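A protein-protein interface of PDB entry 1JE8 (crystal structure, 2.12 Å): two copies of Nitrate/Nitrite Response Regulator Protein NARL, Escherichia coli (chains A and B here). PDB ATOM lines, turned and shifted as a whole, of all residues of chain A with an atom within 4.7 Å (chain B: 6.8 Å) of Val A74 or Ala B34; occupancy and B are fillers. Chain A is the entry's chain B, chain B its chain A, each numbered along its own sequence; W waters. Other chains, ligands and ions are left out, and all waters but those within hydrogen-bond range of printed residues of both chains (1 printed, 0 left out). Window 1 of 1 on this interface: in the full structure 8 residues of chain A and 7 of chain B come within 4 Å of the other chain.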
ATOM      1  N   VAL A  70     -14.106  17.471 -30.283  1.00  0.00           N
ATOM      2  CA  VAL A  70     -12.779  16.971 -29.915  1.00  0.00           C
ATOM      3  C   VAL A  70     -12.810  15.444 -29.781  1.00  0.00           C
ATOM      4  O   VAL A  70     -11.883  14.766 -30.215  1.00  0.00           O
ATOM      5  CB  VAL A  70     -12.280  17.582 -28.594  1.00  0.00           C
ATOM      6  CG1 VAL A  70     -10.811  17.218 -28.373  1.00  0.00           C
ATOM      7  CG2 VAL A  70     -12.458  19.093 -28.627  1.00  0.00           C
ATOM      8  N   GLU A  71     -13.863  14.902 -29.164  1.00  0.00           N
ATOM      9  CA  GLU A  71     -14.003  13.447 -29.044  1.00  0.00           C
ATOM     10  C   GLU A  71     -14.080  12.888 -30.459  1.00  0.00           C
ATOM     11  O   GLU A  71     -13.462  11.865 -30.768  1.00  0.00           O
ATOM     12  CB  GLU A  71     -15.285  13.061 -28.316  1.00  0.00           C
ATOM     13  CG  GLU A  71     -15.338  13.477 -26.878  1.00  0.00           C
ATOM     14  CD  GLU A  71     -16.167  12.517 -26.064  1.00  0.00           C
ATOM     15  OE1 GLU A  71     -17.089  11.909 -26.644  1.00  0.00           O
ATOM     16  OE2 GLU A  71     -15.902  12.383 -24.857  1.00  0.00           O
ATOM     17  N   ALA A  72     -14.848  13.563 -31.315  1.00  0.00           N
ATOM     18  CA  ALA A  72     -14.986  13.136 -32.705  1.00  0.00           C
ATOM     19  C   ALA A  72     -13.622  13.049 -33.396  1.00  0.00           C
ATOM     20  O   ALA A  72     -13.346  12.102 -34.133  1.00  0.00           O
ATOM     21  CB  ALA A  72     -15.910  14.102 -33.465  1.00  0.00           C
ATOM     22  N   ALA A  73     -12.770  14.039 -33.138  1.00  0.00           N
ATOM     23  CA  ALA A  73     -11.439  14.094 -33.739  1.00  0.00           C
ATOM     24  C   ALA A  73     -10.527  13.009 -33.180  1.00  0.00           C
ATOM     25  O   ALA A  73      -9.815  12.337 -33.932  1.00  0.00           O
ATOM     26  CB  ALA A  73     -10.832  15.450 -33.499  1.00  0.00           C
ATOM     27  N   VAL A  74     -10.547  12.838 -31.865  1.00  0.00           N
ATOM     28  CA  VAL A  74      -9.720  11.819 -31.242  1.00  0.00           C
ATOM     29  C   VAL A  74     -10.156  10.422 -31.698  1.00  0.00           C
ATOM     30  O   VAL A  74      -9.321   9.596 -32.061  1.00  0.00           O
ATOM     31  CB  VAL A  74      -9.793  11.919 -29.711  1.00  0.00           C
ATOM     32  CG1 VAL A  74      -9.072  10.736 -29.084  1.00  0.00           C
ATOM     33  CG2 VAL A  74      -9.170  13.235 -29.245  1.00  0.00           C
ATOM     34  N   TRP A  75     -11.466  10.169 -31.689  1.00  0.00           N
ATOM     35  CA  TRP A  75     -12.038   8.891 -32.123  1.00  0.00           C
ATOM     36  C   TRP A  75     -11.541   8.546 -33.528  1.00  0.00           C
ATOM     37  O   TRP A  75     -11.040   7.444 -33.774  1.00  0.00           O
ATOM     38  CB  TRP A  75     -13.572   8.983 -32.120  1.00  0.00           C
ATOM     39  CG  TRP A  75     -14.274   7.824 -32.755  1.00  0.00           C
ATOM     40  CD1 TRP A  75     -14.158   6.506 -32.419  1.00  0.00           C
ATOM     41  CD2 TRP A  75     -15.187   7.878 -33.859  1.00  0.00           C
ATOM     42  NE1 TRP A  75     -14.935   5.735 -33.252  1.00  0.00           N
ATOM     43  CE2 TRP A  75     -15.570   6.551 -34.148  1.00  0.00           C
ATOM     44  CE3 TRP A  75     -15.703   8.917 -34.642  1.00  0.00           C
ATOM     45  CZ2 TRP A  75     -16.459   6.239 -35.183  1.00  0.00           C
ATOM     46  CZ3 TRP A  75     -16.585   8.604 -35.670  1.00  0.00           C
ATOM     47  CH2 TRP A  75     -16.948   7.273 -35.933  1.00  0.00           C
ATOM     48  N   VAL A  76     -11.678   9.489 -34.450  1.00  0.00           N
ATOM     49  CA  VAL A  76     -11.231   9.272 -35.821  1.00  0.00           C
ATOM     50  C   VAL A  76      -9.760   8.845 -35.908  1.00  0.00           C
ATOM     51  O   VAL A  76      -9.396   7.998 -36.731  1.00  0.00           O
ATOM     52  CB  VAL A  76     -11.423  10.548 -36.671  1.00  0.00           C
ATOM     53  CG1 VAL A  76     -10.666  10.423 -37.988  1.00  0.00           C
ATOM     54  CG2 VAL A  76     -12.898  10.780 -36.942  1.00  0.00           C
ATOM     55  N   HIS A  77      -8.914   9.438 -35.065  1.00  0.00           N
ATOM     56  CA  HIS A  77      -7.496   9.109 -35.081  1.00  0.00           C
ATOM     57  C   HIS A  77      -7.181   7.803 -34.390  1.00  0.00           C
ATOM     58  O   HIS A  77      -6.344   7.040 -34.860  1.00  0.00           O
ATOM     59  CB  HIS A  77      -6.667  10.232 -34.463  1.00  0.00           C
ATOM     60  CG  HIS A  77      -6.462  11.396 -35.379  1.00  0.00           C
ATOM     61  ND1 HIS A  77      -7.454  12.312 -35.656  1.00  0.00           N
ATOM     62  CD2 HIS A  77      -5.390  11.769 -36.117  1.00  0.00           C
ATOM     63  CE1 HIS A  77      -7.003  13.199 -36.524  1.00  0.00           C
ATOM     64  NE2 HIS A  77      -5.753  12.892 -36.820  1.00  0.00           N
ATOM     65  N   GLN A  78      -7.851   7.542 -33.275  1.00  0.00           N
ATOM     66  CA  GLN A  78      -7.630   6.306 -32.540  1.00  0.00           C
ATOM     67  C   GLN A  78      -8.101   5.081 -33.319  1.00  0.00           C
ATOM     68  O   GLN A  78      -7.361   4.110 -33.464  1.00  0.00           O
ATOM     69  CB  GLN A  78      -8.339   6.358 -31.190  1.00  0.00           C
ATOM     70  CG  GLN A  78      -7.799   7.420 -30.260  1.00  0.00           C
ATOM     71  CD  GLN A  78      -8.250   7.202 -28.833  1.00  0.00           C
ATOM     72  OE1 GLN A  78      -9.446   7.074 -28.564  1.00  0.00           O
ATOM     73  NE2 GLN A  78      -7.298   7.155 -27.905  1.00  0.00           N
ATOM     74  N   ILE B  29      -1.950  18.620 -19.164  1.00  0.00           N
ATOM     75  CA  ILE B  29      -3.168  19.114 -19.811  1.00  0.00           C
ATOM     76  C   ILE B  29      -3.243  18.688 -21.277  1.00  0.00           C
ATOM     77  O   ILE B  29      -4.288  18.247 -21.749  1.00  0.00           O
ATOM     78  CB  ILE B  29      -3.290  20.678 -19.692  1.00  0.00           C
ATOM     79  CG1 ILE B  29      -3.907  21.063 -18.338  1.00  0.00           C
ATOM     80  CG2 ILE B  29      -4.180  21.235 -20.790  1.00  0.00           C
ATOM     81  CD1 ILE B  29      -3.040  20.786 -17.151  1.00  0.00           C
ATOM     82  N   LEU B  30      -2.141  18.810 -22.001  1.00  0.00           N
ATOM     83  CA  LEU B  30      -2.142  18.407 -23.406  1.00  0.00           C
ATOM     84  C   LEU B  30      -2.514  16.929 -23.570  1.00  0.00           C
ATOM     85  O   LEU B  30      -3.214  16.560 -24.521  1.00  0.00           O
ATOM     86  CB  LEU B  30      -0.775  18.668 -24.030  1.00  0.00           C
ATOM     87  CG  LEU B  30      -0.583  18.276 -25.494  1.00  0.00           C
ATOM     88  CD1 LEU B  30      -1.609  18.972 -26.379  1.00  0.00           C
ATOM     89  CD2 LEU B  30       0.837  18.649 -25.916  1.00  0.00           C
ATOM     90  N   LYS B  31      -2.039  16.078 -22.662  1.00  0.00           N
ATOM     91  CA  LYS B  31      -2.355  14.652 -22.722  1.00  0.00           C
ATOM     92  C   LYS B  31      -3.853  14.453 -22.549  1.00  0.00           C
ATOM     93  O   LYS B  31      -4.475  13.685 -23.284  1.00  0.00           O
ATOM     94  CB  LYS B  31      -1.615  13.908 -21.624  1.00  0.00           C
ATOM     95  CG  LYS B  31      -0.147  13.734 -21.927  1.00  0.00           C
ATOM     96  CD  LYS B  31       0.609  13.104 -20.764  1.00  0.00           C
ATOM     97  CE  LYS B  31       2.086  12.903 -21.126  1.00  0.00           C
ATOM     98  NZ  LYS B  31       2.914  12.467 -19.965  1.00  0.00           N
ATOM     99  N   LEU B  32      -4.436  15.136 -21.570  1.00  0.00           N
ATOM    100  CA  LEU B  32      -5.865  15.006 -21.354  1.00  0.00           C
ATOM    101  C   LEU B  32      -6.700  15.595 -22.504  1.00  0.00           C
ATOM    102  O   LEU B  32      -7.783  15.085 -22.809  1.00  0.00           O
ATOM    103  CB  LEU B  32      -6.228  15.626 -20.012  1.00  0.00           C
ATOM    104  CG  LEU B  32      -6.136  14.689 -18.800  1.00  0.00           C
ATOM    105  CD1 LEU B  32      -5.192  13.548 -19.091  1.00  0.00           C
ATOM    106  CD2 LEU B  32      -5.698  15.468 -17.567  1.00  0.00           C
ATOM    107  N   ILE B  33      -6.212  16.665 -23.136  1.00  0.00           N
ATOM    108  CA  ILE B  33      -6.906  17.256 -24.283  1.00  0.00           C
ATOM    109  C   ILE B  33      -6.905  16.228 -25.415  1.00  0.00           C
ATOM    110  O   ILE B  33      -7.916  16.015 -26.081  1.00  0.00           O
ATOM    111  CB  ILE B  33      -6.204  18.567 -24.760  1.00  0.00           C
ATOM    112  CG1 ILE B  33      -6.604  19.727 -23.835  1.00  0.00           C
ATOM    113  CG2 ILE B  33      -6.579  18.885 -26.199  1.00  0.00           C
ATOM    114  CD1 ILE B  33      -5.926  21.008 -24.154  1.00  0.00           C
ATOM    115  N   ALA B  34      -5.763  15.577 -25.617  1.00  0.00           N
ATOM    116  CA  ALA B  34      -5.631  14.572 -26.663  1.00  0.00           C
ATOM    117  C   ALA B  34      -6.549  13.389 -26.398  1.00  0.00           C
ATOM    118  O   ALA B  34      -6.768  12.570 -27.276  1.00  0.00           O
ATOM    119  CB  ALA B  34      -4.196  14.104 -26.764  1.00  0.00           C
ATOM    120  N   GLN B  35      -7.083  13.301 -25.187  1.00  0.00           N
ATOM    121  CA  GLN B  35      -8.004  12.226 -24.844  1.00  0.00           C
ATOM    122  C   GLN B  35      -9.432  12.744 -24.927  1.00  0.00           C
ATOM    123  O   GLN B  35     -10.355  12.097 -24.438  1.00  0.00           O
ATOM    124  CB  GLN B  35      -7.730  11.720 -23.437  1.00  0.00           C
ATOM    125  CG  GLN B  35      -6.561  10.791 -23.386  1.00  0.00           C
ATOM    126  CD  GLN B  35      -5.985  10.693 -22.013  1.00  0.00           C
ATOM    127  OE1 GLN B  35      -6.690  10.398 -21.050  1.00  0.00           O
ATOM    128  NE2 GLN B  35      -4.693  10.945 -21.904  1.00  0.00           N
ATOM    129  N   GLY B  36      -9.580  13.933 -25.518  1.00  0.00           N
ATOM    130  CA  GLY B  36     -10.875  14.579 -25.722  1.00  0.00           C
ATOM    131  C   GLY B  36     -11.646  15.131 -24.538  1.00  0.00           C
ATOM    132  O   GLY B  36     -12.870  15.223 -24.592  1.00  0.00           O
ATOM    133  N   LEU B  37     -10.945  15.520 -23.475  1.00  0.00           N
ATOM    134  CA  LEU B  37     -11.594  16.032 -22.275  1.00  0.00           C
ATOM    135  C   LEU B  37     -11.751  17.534 -22.266  1.00  0.00           C
ATOM    136  O   LEU B  37     -10.825  18.272 -22.620  1.00  0.00           O
ATOM    137  CB  LEU B  37     -10.814  15.622 -21.017  1.00  0.00           C
ATOM    138  CG  LEU B  37     -11.039  14.209 -20.463  1.00  0.00           C
ATOM    139  CD1 LEU B  37     -10.725  13.167 -21.526  1.00  0.00           C
ATOM    140  CD2 LEU B  37     -10.153  13.985 -19.250  1.00  0.00           C
ATOM    141  N   ARG B  69      -7.627  23.771 -29.108  1.00  0.00           N
ATOM    142  CA  ARG B  69      -7.393  22.489 -28.457  1.00  0.00           C
ATOM    143  C   ARG B  69      -7.584  21.338 -29.457  1.00  0.00           C
ATOM    144  O   ARG B  69      -6.974  20.276 -29.319  1.00  0.00           O
ATOM    145  CB  ARG B  69      -8.340  22.316 -27.266  1.00  0.00           C
ATOM    146  CG  ARG B  69      -9.800  22.216 -27.639  1.00  0.00           C
ATOM    147  CD  ARG B  69     -10.677  22.642 -26.472  1.00  0.00           C
ATOM    148  NE  ARG B  69     -10.570  21.739 -25.320  1.00  0.00           N
ATOM    149  CZ  ARG B  69     -10.085  22.095 -24.132  1.00  0.00           C
ATOM    150  NH1 ARG B  69      -9.656  23.336 -23.929  1.00  0.00           N
ATOM    151  NH2 ARG B  69     -10.047  21.222 -23.134  1.00  0.00           N
ATOM    152  N   ALA B  72      -4.434  20.896 -31.146  1.00  0.00           N
ATOM    153  CA  ALA B  72      -3.583  20.255 -30.164  1.00  0.00           C
ATOM    154  C   ALA B  72      -3.806  18.740 -30.116  1.00  0.00           C
ATOM    155  O   ALA B  72      -2.838  17.977 -30.074  1.00  0.00           O
ATOM    156  CB  ALA B  72      -3.830  20.854 -28.806  1.00  0.00           C
ATOM    157  N   ALA B  73      -5.074  18.313 -30.111  1.00  0.00           N
ATOM    158  CA  ALA B  73      -5.432  16.887 -30.060  1.00  0.00           C
ATOM    159  C   ALA B  73      -5.008  16.160 -31.333  1.00  0.00           C
ATOM    160  O   ALA B  73      -4.400  15.087 -31.284  1.00  0.00           O
ATOM    161  CB  ALA B  73      -6.937  16.731 -29.853  1.00  0.00           C
ATOM    162  N   VAL B  74      -5.329  16.755 -32.476  1.00  0.00           N
ATOM    163  CA  VAL B  74      -4.975  16.174 -33.763  1.00  0.00           C
ATOM    164  C   VAL B  74      -3.449  16.068 -33.883  1.00  0.00           C
ATOM    165  O   VAL B  74      -2.911  15.011 -34.214  1.00  0.00           O
ATOM    166  CB  VAL B  74      -5.537  17.030 -34.918  1.00  0.00           C
ATOM    167  CG1 VAL B  74      -4.958  16.566 -36.234  1.00  0.00           C
ATOM    168  CG2 VAL B  74      -7.059  16.918 -34.948  1.00  0.00           C
ATOM    169  N   VAL B  76      -1.222  15.906 -31.593  1.00  0.00           N
ATOM    170  CA  VAL B  76      -0.718  14.852 -30.709  1.00  0.00           C
ATOM    171  C   VAL B  76      -0.861  13.447 -31.306  1.00  0.00           C
ATOM    172  O   VAL B  76       0.012  12.601 -31.124  1.00  0.00           O
ATOM    173  CB  VAL B  76      -1.452  14.862 -29.336  1.00  0.00           C
ATOM    174  CG1 VAL B  76      -1.142  13.580 -28.554  1.00  0.00           C
ATOM    175  CG2 VAL B  76      -1.035  16.086 -28.517  1.00  0.00           C
ATOM    176  N   HIS B  77      -1.972  13.187 -31.997  1.00  0.00           N
ATOM    177  CA  HIS B  77      -2.214  11.873 -32.592  1.00  0.00           C
ATOM    178  C   HIS B  77      -1.422  11.640 -33.870  1.00  0.00           C
ATOM    179  O   HIS B  77      -1.062  10.506 -34.196  1.00  0.00           O
ATOM    180  CB  HIS B  77      -3.712  11.683 -32.824  1.00  0.00           C
ATOM    181  CG  HIS B  77      -4.469  11.402 -31.565  1.00  0.00           C
ATOM    182  ND1 HIS B  77      -4.578  10.141 -31.034  1.00  0.00           N
ATOM    183  CD2 HIS B  77      -5.086  12.237 -30.695  1.00  0.00           C
ATOM    184  CE1 HIS B  77      -5.234  10.204 -29.883  1.00  0.00           C
ATOM    185  NE2 HIS B  77      -5.548  11.464 -29.659  1.00  0.00           N
ATOM    186  N   PHE B  82       3.673  11.518 -26.824  1.00  0.00           N
ATOM    187  CA  PHE B  82       3.217  10.778 -25.653  1.00  0.00           C
ATOM    188  C   PHE B  82       3.068   9.282 -25.951  1.00  0.00           C
ATOM    189  O   PHE B  82       3.154   8.889 -27.139  1.00  0.00           O
ATOM    190  CB  PHE B  82       1.870  11.317 -25.159  1.00  0.00           C
ATOM    191  CG  PHE B  82       1.879  12.792 -24.904  1.00  0.00           C
ATOM    192  CD1 PHE B  82       2.922  13.384 -24.201  1.00  0.00           C
ATOM    193  CD2 PHE B  82       0.791  13.568 -25.271  1.00  0.00           C
ATOM    194  CE1 PHE B  82       2.925  14.749 -23.947  1.00  0.00           C
ATOM    195  CE2 PHE B  82       0.783  14.930 -25.022  1.00  0.00           C
ATOM    196  CZ  PHE B  82       1.837  15.517 -24.320  1.00  0.00           C
ATOM    197  OXT PHE B  82       2.852   8.523 -24.979  1.00  0.00           O
HETATM  198  O   HOH W   1     -15.099  14.327 -23.511  1.00  0.00           O
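Water W1 lies within hydrogen-bond range of the side-chain carboxylate (OE2) of Glu A71 (2.5 Å) and the backbone carbonyl oxygen (O) of Gly B36 (2.6 Å).
O of Ala B34 is in hydrogen-bond range of NE2 of His B77, 2.9 Å away.
O of Ala A73 lies within hydrogen-bond range of ND1 of His A77, 2.9 Å away.
Val A74 touches His B77, and with the chains exchanged His A77 touches Val B74.
His A77 touches its own counterpart, His B77.
Of the 9 pairs that touch across the chains among the printed residues, 3 have their exchanged pair printed and touching as well.
Hydrophobic or aromatic side chains of chain B within 4 Å of the printed part of chain A: Val B74 and His B77.
Of the 9 printed residues of chain A, 5 touch a printed residue of chain B.
Hydrophobic or aromatic side chains of chain A within 4 Å of the printed part of chain B: Val A70, Val A74 and His A77.
Among the printed residues, 9 pairs touch across the chains.
Among the printed residues, no Asp or Glu carboxylate lies within 4 Å of a Lys or Arg side-chain nitrogen of the other chain.
Printed residues of chain B within 4 Å of Val A74: Ala B34, Gly B36 and His B77.
Ala B34 touches one residue of chain A.
Printed residues of chain A within 4 Å of His B77: Val A74, His A77 and Gln A78.
Printed residues of chain B within 4 Å of Glu A71: Gly B36.
Ala A72 touches none of the printed residues of chain B.
Leu B37 touches none of the printed residues of chain A.
The nearest printed residue of chain A that does not touch Ile B33 is Val A74 (4.4 Å).
Val A70 touches Ile B33.
Val A70 touches Gly B36 (CG1 to CA, 3.7 Å).
Gly B36 touches Glu A71.
Ala B34 touches Val A74.
Val A74 touches Gly B36 (CG2 to N, 3.8 Å).
His B77 touches Val A74.
Val B74 touches His A77.
His B77 touches His A77.
Gln A78 touches His B77.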
